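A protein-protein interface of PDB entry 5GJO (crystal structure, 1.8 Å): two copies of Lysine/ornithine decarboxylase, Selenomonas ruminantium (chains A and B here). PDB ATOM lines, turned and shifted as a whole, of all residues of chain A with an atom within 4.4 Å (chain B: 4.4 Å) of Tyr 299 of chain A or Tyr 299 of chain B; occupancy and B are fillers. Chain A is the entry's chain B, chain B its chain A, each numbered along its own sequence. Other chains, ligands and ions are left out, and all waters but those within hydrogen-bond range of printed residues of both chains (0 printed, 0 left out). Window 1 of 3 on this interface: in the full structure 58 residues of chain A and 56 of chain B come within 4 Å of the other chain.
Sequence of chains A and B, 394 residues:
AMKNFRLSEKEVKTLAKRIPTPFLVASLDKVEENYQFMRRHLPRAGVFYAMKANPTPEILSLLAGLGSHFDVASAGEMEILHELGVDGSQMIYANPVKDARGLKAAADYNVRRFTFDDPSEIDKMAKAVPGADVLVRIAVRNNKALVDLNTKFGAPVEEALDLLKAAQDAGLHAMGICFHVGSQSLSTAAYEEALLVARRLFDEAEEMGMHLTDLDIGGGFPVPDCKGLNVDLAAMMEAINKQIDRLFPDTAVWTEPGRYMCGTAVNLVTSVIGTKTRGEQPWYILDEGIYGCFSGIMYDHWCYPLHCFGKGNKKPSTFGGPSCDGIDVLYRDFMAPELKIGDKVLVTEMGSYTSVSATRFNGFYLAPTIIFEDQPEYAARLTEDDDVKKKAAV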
ATOM      1  N   ILE A 290      24.422   2.244  29.351  1.00  0.00           N
ATOM      2  CA  ILE A 290      24.623   1.012  28.634  1.00  0.00           C
ATOM      3  C   ILE A 290      23.921  -0.175  29.293  1.00  0.00           C
ATOM      4  O   ILE A 290      23.711  -1.259  28.663  1.00  0.00           O
ATOM      5  CB  ILE A 290      26.170   0.771  28.467  1.00  0.00           C
ATOM      6  CG1 ILE A 290      26.464  -0.053  27.229  1.00  0.00           C
ATOM      7  CG2 ILE A 290      26.774   0.144  29.697  1.00  0.00           C
ATOM      8  CD1 ILE A 290      27.875  -0.089  26.787  1.00  0.00           C
ATOM      9  N   TYR A 291      23.596  -0.018  30.558  1.00  0.00           N
ATOM     10  CA  TYR A 291      22.799  -1.048  31.305  1.00  0.00           C
ATOM     11  C   TYR A 291      21.260  -0.858  31.221  1.00  0.00           C
ATOM     12  O   TYR A 291      20.480  -1.678  31.722  1.00  0.00           O
ATOM     13  CB  TYR A 291      23.209  -1.129  32.797  1.00  0.00           C
ATOM     14  CG  TYR A 291      24.529  -1.759  32.990  1.00  0.00           C
ATOM     15  CD1 TYR A 291      24.653  -3.157  32.941  1.00  0.00           C
ATOM     16  CD2 TYR A 291      25.641  -1.019  33.186  1.00  0.00           C
ATOM     17  CE1 TYR A 291      25.840  -3.770  33.158  1.00  0.00           C
ATOM     18  CE2 TYR A 291      26.907  -1.640  33.343  1.00  0.00           C
ATOM     19  CZ  TYR A 291      26.972  -3.042  33.376  1.00  0.00           C
ATOM     20  OH  TYR A 291      28.195  -3.661  33.565  1.00  0.00           O
ATOM     21  N   SER A 295      21.789  -0.528  26.020  1.00  0.00           N
ATOM     22  CA  SER A 295      22.263  -1.888  25.968  1.00  0.00           C
ATOM     23  C   SER A 295      22.406  -2.474  24.572  1.00  0.00           C
ATOM     24  O   SER A 295      23.216  -3.378  24.363  1.00  0.00           O
ATOM     25  CB  SER A 295      21.313  -2.782  26.768  1.00  0.00           C
ATOM     26  OG  SER A 295      20.005  -2.723  26.274  1.00  0.00           O
ATOM     27  N   GLY A 296      21.681  -1.916  23.604  1.00  0.00           N
ATOM     28  CA  GLY A 296      21.884  -2.278  22.224  1.00  0.00           C
ATOM     29  C   GLY A 296      23.264  -1.989  21.643  1.00  0.00           C
ATOM     30  O   GLY A 296      23.656  -2.674  20.711  1.00  0.00           O
ATOM     31  N   ILE A 297      24.038  -1.088  22.268  1.00  0.00           N
ATOM     32  CA  ILE A 297      25.387  -0.899  21.911  1.00  0.00           C
ATOM     33  C   ILE A 297      26.127  -2.233  22.065  1.00  0.00           C
ATOM     34  O   ILE A 297      27.012  -2.567  21.254  1.00  0.00           O
ATOM     35  CB  ILE A 297      26.101   0.196  22.763  1.00  0.00           C
ATOM     36  CG1 ILE A 297      25.445   1.562  22.471  1.00  0.00           C
ATOM     37  CG2 ILE A 297      27.595   0.282  22.453  1.00  0.00           C
ATOM     38  CD1 ILE A 297      26.031   2.654  23.387  1.00  0.00           C
ATOM     39  N   MET A 298      25.857  -2.900  23.165  1.00  0.00           N
ATOM     40  CA  MET A 298      26.500  -4.151  23.483  1.00  0.00           C
ATOM     41  C   MET A 298      25.941  -5.402  22.808  1.00  0.00           C
ATOM     42  O   MET A 298      26.670  -6.146  22.222  1.00  0.00           O
ATOM     43  CB  MET A 298      26.486  -4.318  24.992  1.00  0.00           C
ATOM     44  CG  MET A 298      27.242  -3.203  25.693  1.00  0.00           C
ATOM     45  SD  MET A 298      29.022  -3.397  25.555  1.00  0.00           S
ATOM     46  CE  MET A 298      29.107  -5.189  25.712  1.00  0.00           C
ATOM     47  N   TYR A 299      24.635  -5.600  22.894  1.00  0.00           N
ATOM     48  CA  TYR A 299      24.005  -6.804  22.381  1.00  0.00           C
ATOM     49  C   TYR A 299      23.607  -6.737  20.874  1.00  0.00           C
ATOM     50  O   TYR A 299      23.441  -7.740  20.258  1.00  0.00           O
ATOM     51  CB  TYR A 299      22.755  -7.160  23.157  1.00  0.00           C
ATOM     52  CG  TYR A 299      23.038  -7.676  24.503  1.00  0.00           C
ATOM     53  CD1 TYR A 299      23.431  -8.978  24.687  1.00  0.00           C
ATOM     54  CD2 TYR A 299      22.842  -6.906  25.607  1.00  0.00           C
ATOM     55  CE1 TYR A 299      23.632  -9.524  25.948  1.00  0.00           C
ATOM     56  CE2 TYR A 299      23.125  -7.411  26.863  1.00  0.00           C
ATOM     57  CZ  TYR A 299      23.498  -8.769  27.036  1.00  0.00           C
ATOM     58  OH  TYR A 299      23.735  -9.312  28.338  1.00  0.00           O
ATOM     59  N   ASP A 300      23.446  -5.537  20.368  1.00  0.00           N
ATOM     60  CA  ASP A 300      22.891  -5.383  19.036  1.00  0.00           C
ATOM     61  C   ASP A 300      23.888  -4.645  18.111  1.00  0.00           C
ATOM     62  O   ASP A 300      23.471  -4.192  17.022  1.00  0.00           O
ATOM     63  CB  ASP A 300      21.559  -4.627  19.179  1.00  0.00           C
ATOM     64  CG  ASP A 300      20.679  -4.689  17.909  1.00  0.00           C
ATOM     65  OD1 ASP A 300      20.522  -5.778  17.295  1.00  0.00           O
ATOM     66  OD2 ASP A 300      20.020  -3.640  17.599  1.00  0.00           O
ATOM     67  N   HIS A 301      25.129  -4.380  18.596  1.00  0.00           N
ATOM     68  CA  HIS A 301      26.179  -3.770  17.786  1.00  0.00           C
ATOM     69  C   HIS A 301      25.795  -2.407  17.271  1.00  0.00           C
ATOM     70  O   HIS A 301      26.250  -2.029  16.197  1.00  0.00           O
ATOM     71  CB  HIS A 301      26.557  -4.694  16.645  1.00  0.00           C
ATOM     72  CG  HIS A 301      26.830  -6.094  17.102  1.00  0.00           C
ATOM     73  ND1 HIS A 301      26.159  -7.195  16.603  1.00  0.00           N
ATOM     74  CD2 HIS A 301      27.615  -6.557  18.102  1.00  0.00           C
ATOM     75  CE1 HIS A 301      26.566  -8.280  17.238  1.00  0.00           C
ATOM     76  NE2 HIS A 301      27.449  -7.925  18.151  1.00  0.00           N
ATOM     77  N   ILE A 327      32.680   0.503  31.783  1.00  0.00           N
ATOM     78  CA  ILE A 327      32.141   0.147  30.472  1.00  0.00           C
ATOM     79  C   ILE A 327      31.006   1.057  29.976  1.00  0.00           C
ATOM     80  O   ILE A 327      30.640   1.008  28.840  1.00  0.00           O
ATOM     81  CB  ILE A 327      31.698  -1.325  30.418  1.00  0.00           C
ATOM     82  CG1 ILE A 327      31.718  -1.848  28.996  1.00  0.00           C
ATOM     83  CG2 ILE A 327      30.340  -1.519  31.034  1.00  0.00           C
ATOM     84  CD1 ILE A 327      31.487  -3.336  28.947  1.00  0.00           C
ATOM     85  N   SER A 357      16.385  -5.083  26.500  1.00  0.00           N
ATOM     86  CA  SER A 357      17.633  -5.643  27.105  1.00  0.00           C
ATOM     87  C   SER A 357      18.119  -4.704  28.222  1.00  0.00           C
ATOM     88  O   SER A 357      19.223  -4.830  28.738  1.00  0.00           O
ATOM     89  CB  SER A 357      18.684  -5.935  26.004  1.00  0.00           C
ATOM     90  OG  SER A 357      18.927  -4.783  25.218  1.00  0.00           O
ATOM     91  N   ILE B 290      22.904 -15.648  27.639  1.00  0.00           N
ATOM     92  CA  ILE B 290      23.662 -14.405  27.655  1.00  0.00           C
ATOM     93  C   ILE B 290      22.802 -13.189  27.990  1.00  0.00           C
ATOM     94  O   ILE B 290      23.348 -12.163  28.427  1.00  0.00           O
ATOM     95  CB  ILE B 290      24.416 -14.228  26.345  1.00  0.00           C
ATOM     96  CG1 ILE B 290      25.632 -13.312  26.563  1.00  0.00           C
ATOM     97  CG2 ILE B 290      23.484 -13.669  25.272  1.00  0.00           C
ATOM     98  CD1 ILE B 290      26.628 -13.341  25.456  1.00  0.00           C
ATOM     99  N   TYR B 291      21.476 -13.330  27.907  1.00  0.00           N
ATOM    100  CA  TYR B 291      20.580 -12.269  28.348  1.00  0.00           C
ATOM    101  C   TYR B 291      20.105 -12.457  29.776  1.00  0.00           C
ATOM    102  O   TYR B 291      19.305 -11.664  30.249  1.00  0.00           O
ATOM    103  CB  TYR B 291      19.376 -12.137  27.450  1.00  0.00           C
ATOM    104  CG  TYR B 291      19.693 -11.544  26.099  1.00  0.00           C
ATOM    105  CD1 TYR B 291      19.746 -10.175  25.949  1.00  0.00           C
ATOM    106  CD2 TYR B 291      19.894 -12.351  24.960  1.00  0.00           C
ATOM    107  CE1 TYR B 291      20.025  -9.609  24.717  1.00  0.00           C
ATOM    108  CE2 TYR B 291      20.191 -11.746  23.707  1.00  0.00           C
ATOM    109  CZ  TYR B 291      20.218 -10.396  23.625  1.00  0.00           C
ATOM    110  OH  TYR B 291      20.454  -9.737  22.403  1.00  0.00           O
ATOM    111  N   SER B 295      25.062 -12.860  31.203  1.00  0.00           N
ATOM    112  CA  SER B 295      25.336 -11.490  30.741  1.00  0.00           C
ATOM    113  C   SER B 295      26.684 -10.947  31.124  1.00  0.00           C
ATOM    114  O   SER B 295      27.227 -10.105  30.392  1.00  0.00           O
ATOM    115  CB  SER B 295      24.238 -10.510  31.284  1.00  0.00           C
ATOM    116  OG  SER B 295      24.165 -10.613  32.734  1.00  0.00           O
ATOM    117  N   GLY B 296      27.316 -11.482  32.191  1.00  0.00           N
ATOM    118  CA  GLY B 296      28.684 -11.166  32.526  1.00  0.00           C
ATOM    119  C   GLY B 296      29.711 -11.473  31.417  1.00  0.00           C
ATOM    120  O   GLY B 296      30.760 -10.852  31.365  1.00  0.00           O
ATOM    121  N   ILE B 297      29.384 -12.402  30.519  1.00  0.00           N
ATOM    122  CA  ILE B 297      30.208 -12.610  29.323  1.00  0.00           C
ATOM    123  C   ILE B 297      30.376 -11.312  28.613  1.00  0.00           C
ATOM    124  O   ILE B 297      31.474 -11.001  28.089  1.00  0.00           O
ATOM    125  CB  ILE B 297      29.601 -13.702  28.392  1.00  0.00           C
ATOM    126  CG1 ILE B 297      29.701 -15.047  29.102  1.00  0.00           C
ATOM    127  CG2 ILE B 297      30.344 -13.747  27.087  1.00  0.00           C
ATOM    128  CD1 ILE B 297      29.030 -16.163  28.311  1.00  0.00           C
ATOM    129  N   MET B 298      29.283 -10.582  28.492  1.00  0.00           N
ATOM    130  CA  MET B 298      29.225  -9.354  27.696  1.00  0.00           C
ATOM    131  C   MET B 298      29.700  -8.137  28.470  1.00  0.00           C
ATOM    132  O   MET B 298      30.566  -7.358  28.021  1.00  0.00           O
ATOM    133  CB  MET B 298      27.776  -9.144  27.247  1.00  0.00           C
ATOM    134  CG  MET B 298      27.294 -10.211  26.298  1.00  0.00           C
ATOM    135  SD  MET B 298      28.280 -10.179  24.757  1.00  0.00           S
ATOM    136  CE  MET B 298      28.170  -8.288  24.555  1.00  0.00           C
ATOM    137  N   TYR B 299      29.141  -7.928  29.628  1.00  0.00           N
ATOM    138  CA  TYR B 299      29.432  -6.715  30.376  1.00  0.00           C
ATOM    139  C   TYR B 299      30.671  -6.813  31.244  1.00  0.00           C
ATOM    140  O   TYR B 299      31.215  -5.781  31.613  1.00  0.00           O
ATOM    141  CB  TYR B 299      28.265  -6.264  31.267  1.00  0.00           C
ATOM    142  CG  TYR B 299      27.099  -5.727  30.541  1.00  0.00           C
ATOM    143  CD1 TYR B 299      27.081  -4.431  30.103  1.00  0.00           C
ATOM    144  CD2 TYR B 299      25.993  -6.511  30.293  1.00  0.00           C
ATOM    145  CE1 TYR B 299      26.028  -3.950  29.396  1.00  0.00           C
ATOM    146  CE2 TYR B 299      24.905  -5.991  29.608  1.00  0.00           C
ATOM    147  CZ  TYR B 299      24.950  -4.726  29.141  1.00  0.00           C
ATOM    148  OH  TYR B 299      23.847  -4.155  28.500  1.00  0.00           O
ATOM    149  N   ASP B 300      31.062  -7.996  31.639  1.00  0.00           N
ATOM    150  CA  ASP B 300      32.087  -8.188  32.707  1.00  0.00           C
ATOM    151  C   ASP B 300      33.240  -9.000  32.128  1.00  0.00           C
ATOM    152  O   ASP B 300      34.085  -9.449  32.893  1.00  0.00           O
ATOM    153  CB  ASP B 300      31.431  -8.930  33.873  1.00  0.00           C
ATOM    154  CG  ASP B 300      32.220  -8.857  35.176  1.00  0.00           C
ATOM    155  OD1 ASP B 300      32.807  -7.820  35.499  1.00  0.00           O
ATOM    156  OD2 ASP B 300      32.245  -9.907  35.887  1.00  0.00           O
ATOM    157  N   HIS B 301      33.276  -9.154  30.775  1.00  0.00           N
ATOM    158  CA  HIS B 301      34.327  -9.839  30.031  1.00  0.00           C
ATOM    159  C   HIS B 301      34.654 -11.206  30.664  1.00  0.00           C
ATOM    160  O   HIS B 301      35.829 -11.598  30.757  1.00  0.00           O
ATOM    161  CB  HIS B 301      35.633  -8.998  29.965  1.00  0.00           C
ATOM    162  CG  HIS B 301      35.399  -7.551  29.676  1.00  0.00           C
ATOM    163  ND1 HIS B 301      35.817  -6.546  30.539  1.00  0.00           N
ATOM    164  CD2 HIS B 301      34.687  -6.938  28.695  1.00  0.00           C
ATOM    165  CE1 HIS B 301      35.407  -5.376  30.076  1.00  0.00           C
ATOM    166  NE2 HIS B 301      34.725  -5.580  28.956  1.00  0.00           N
ATOM    167  N   ILE B 327      23.770 -14.056  18.983  1.00  0.00           N
ATOM    168  CA  ILE B 327      24.782 -13.732  19.948  1.00  0.00           C
ATOM    169  C   ILE B 327      24.745 -14.640  21.190  1.00  0.00           C
ATOM    170  O   ILE B 327      25.645 -14.629  21.965  1.00  0.00           O
ATOM    171  CB  ILE B 327      24.726 -12.254  20.347  1.00  0.00           C
ATOM    172  CG1 ILE B 327      26.097 -11.768  20.768  1.00  0.00           C
ATOM    173  CG2 ILE B 327      23.696 -12.001  21.424  1.00  0.00           C
ATOM    174  CD1 ILE B 327      26.159 -10.274  20.898  1.00  0.00           C
ATOM    175  N   SER B 357      22.771  -8.132  35.988  1.00  0.00           N
ATOM    176  CA  SER B 357      22.634  -7.639  34.604  1.00  0.00           C
ATOM    177  C   SER B 357      21.770  -8.552  33.747  1.00  0.00           C
ATOM    178  O   SER B 357      21.746  -8.468  32.524  1.00  0.00           O
ATOM    179  CB  SER B 357      23.979  -7.304  33.956  1.00  0.00           C
ATOM    180  OG  SER B 357      24.836  -8.453  34.149  1.00  0.00           O
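O of Ile 290 of chain B is in hydrogen-bond range of OH of Tyr 299 of chain A (2.9 Å).
The side-chain hydroxyl of Tyr 299 of chain B is in hydrogen-bond range of the backbone carbonyl oxygen of Ile 290 of chain A (2.9 Å).
Tyr 291 of chain A touches Tyr 299 of chain B, and with the chains exchanged Tyr 299 of chain A touches Tyr 291 of chain B.
Ser 295 of chain A touches Tyr 299 of chain B, and with the chains exchanged Tyr 299 of chain A touches Ser 295 of chain B.
Met 298 of chain A touches Tyr 299 of chain B, and with the chains exchanged Tyr 299 of chain A touches Met 298 of chain B.
Tyr 299 of chain A touches Ile 327 of chain B, and with the chains exchanged Ile 327 of chain A touches Tyr 299 of chain B.
CE1 of Tyr 291 of chain A touches CD1 of Tyr 299 of chain B, 3.4 Å away.
Ser 295 of chain A touches Tyr 299 of chain B.
Met 298 of chain A touches Met 298 of chain B (CE to CE, 3.4 Å).
CE1 of Tyr 291 of chain B touches CD1 of Tyr 299 of chain A (3.5 Å).
OH of Tyr 299 of chain A touches CB of Ser 295 of chain B (3.2 Å).
Met 298 of chain B touches Tyr 299 of chain A.
O of Tyr 299 of chain A touches CD1 of Ile 327 of chain B, at 3.8 Å.
His 301 of chain A touches Ile 327 of chain B.
Ile 327 of chain A touches Tyr 299 of chain B (CD1 to O, 3.6 Å).
His 301 of chain B touches Ile 327 of chain A.
O of Ile 290 of chain B lies close to N of Ser 295 of chain B.
The side-chain hydroxyl (OG) of Ser 357 of chain B is in hydrogen-bond range of the side-chain hydroxyl (OG) of Ser 295 of chain B, at 2.7 Å.
The backbone carbonyl oxygen (O) of Gly 296 of chain B sits at hydrogen-bond distance from the backbone NH (N) of His 301 of chain B.
The backbone carbonyl oxygen (O) of Ile 290 of chain A lies close to the backbone NH (N) of Ser 295 of chain A (3.3 Å).
The side-chain hydroxyl (OG) of Ser 295 of chain A sits at hydrogen-bond distance from the side-chain hydroxyl (OG) of Ser 357 of chain A (2.6 Å).
The backbone carbonyl oxygen (O) of Gly 296 of chain A lies within hydrogen-bond range of the backbone NH (N) of His 301 of chain A (3.1 Å).
Tyr 299 of chain A touches six residues of chain B.
Tyr 299 of chain B touches just these residues of chain A: Ile 290, Tyr 291, Ser 295, Met 298, Tyr 299 and Ile 327.
Printed residues of chain B within 4 Å of Met 298 of chain A: Met 298 and Tyr 299.
Of the printed residues of chain A, His 301 of chain B touches Ile 327.
Of the printed residues of chain B, Tyr 291 of chain A touches Tyr 299 (3.4 Å).
Printed residues of chain B within 4 Å of Ser 295 of chain A: Tyr 299 (3.4 Å).
Gly 296 of chain A touches none of the printed residues of chain B.
Asp 300 of chain B touches none of the printed residues of chain A.
The nearest printed residue of chain A that does not touch Ser 295 of chain B is Met 298 of chain A (7.0 Å).
Among the printed residues, 14 pairs touch across the chains.
Among the printed residues, no Asp or Glu carboxylate lies within 4 Å of a Lys or Arg side-chain nitrogen of the other chain.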
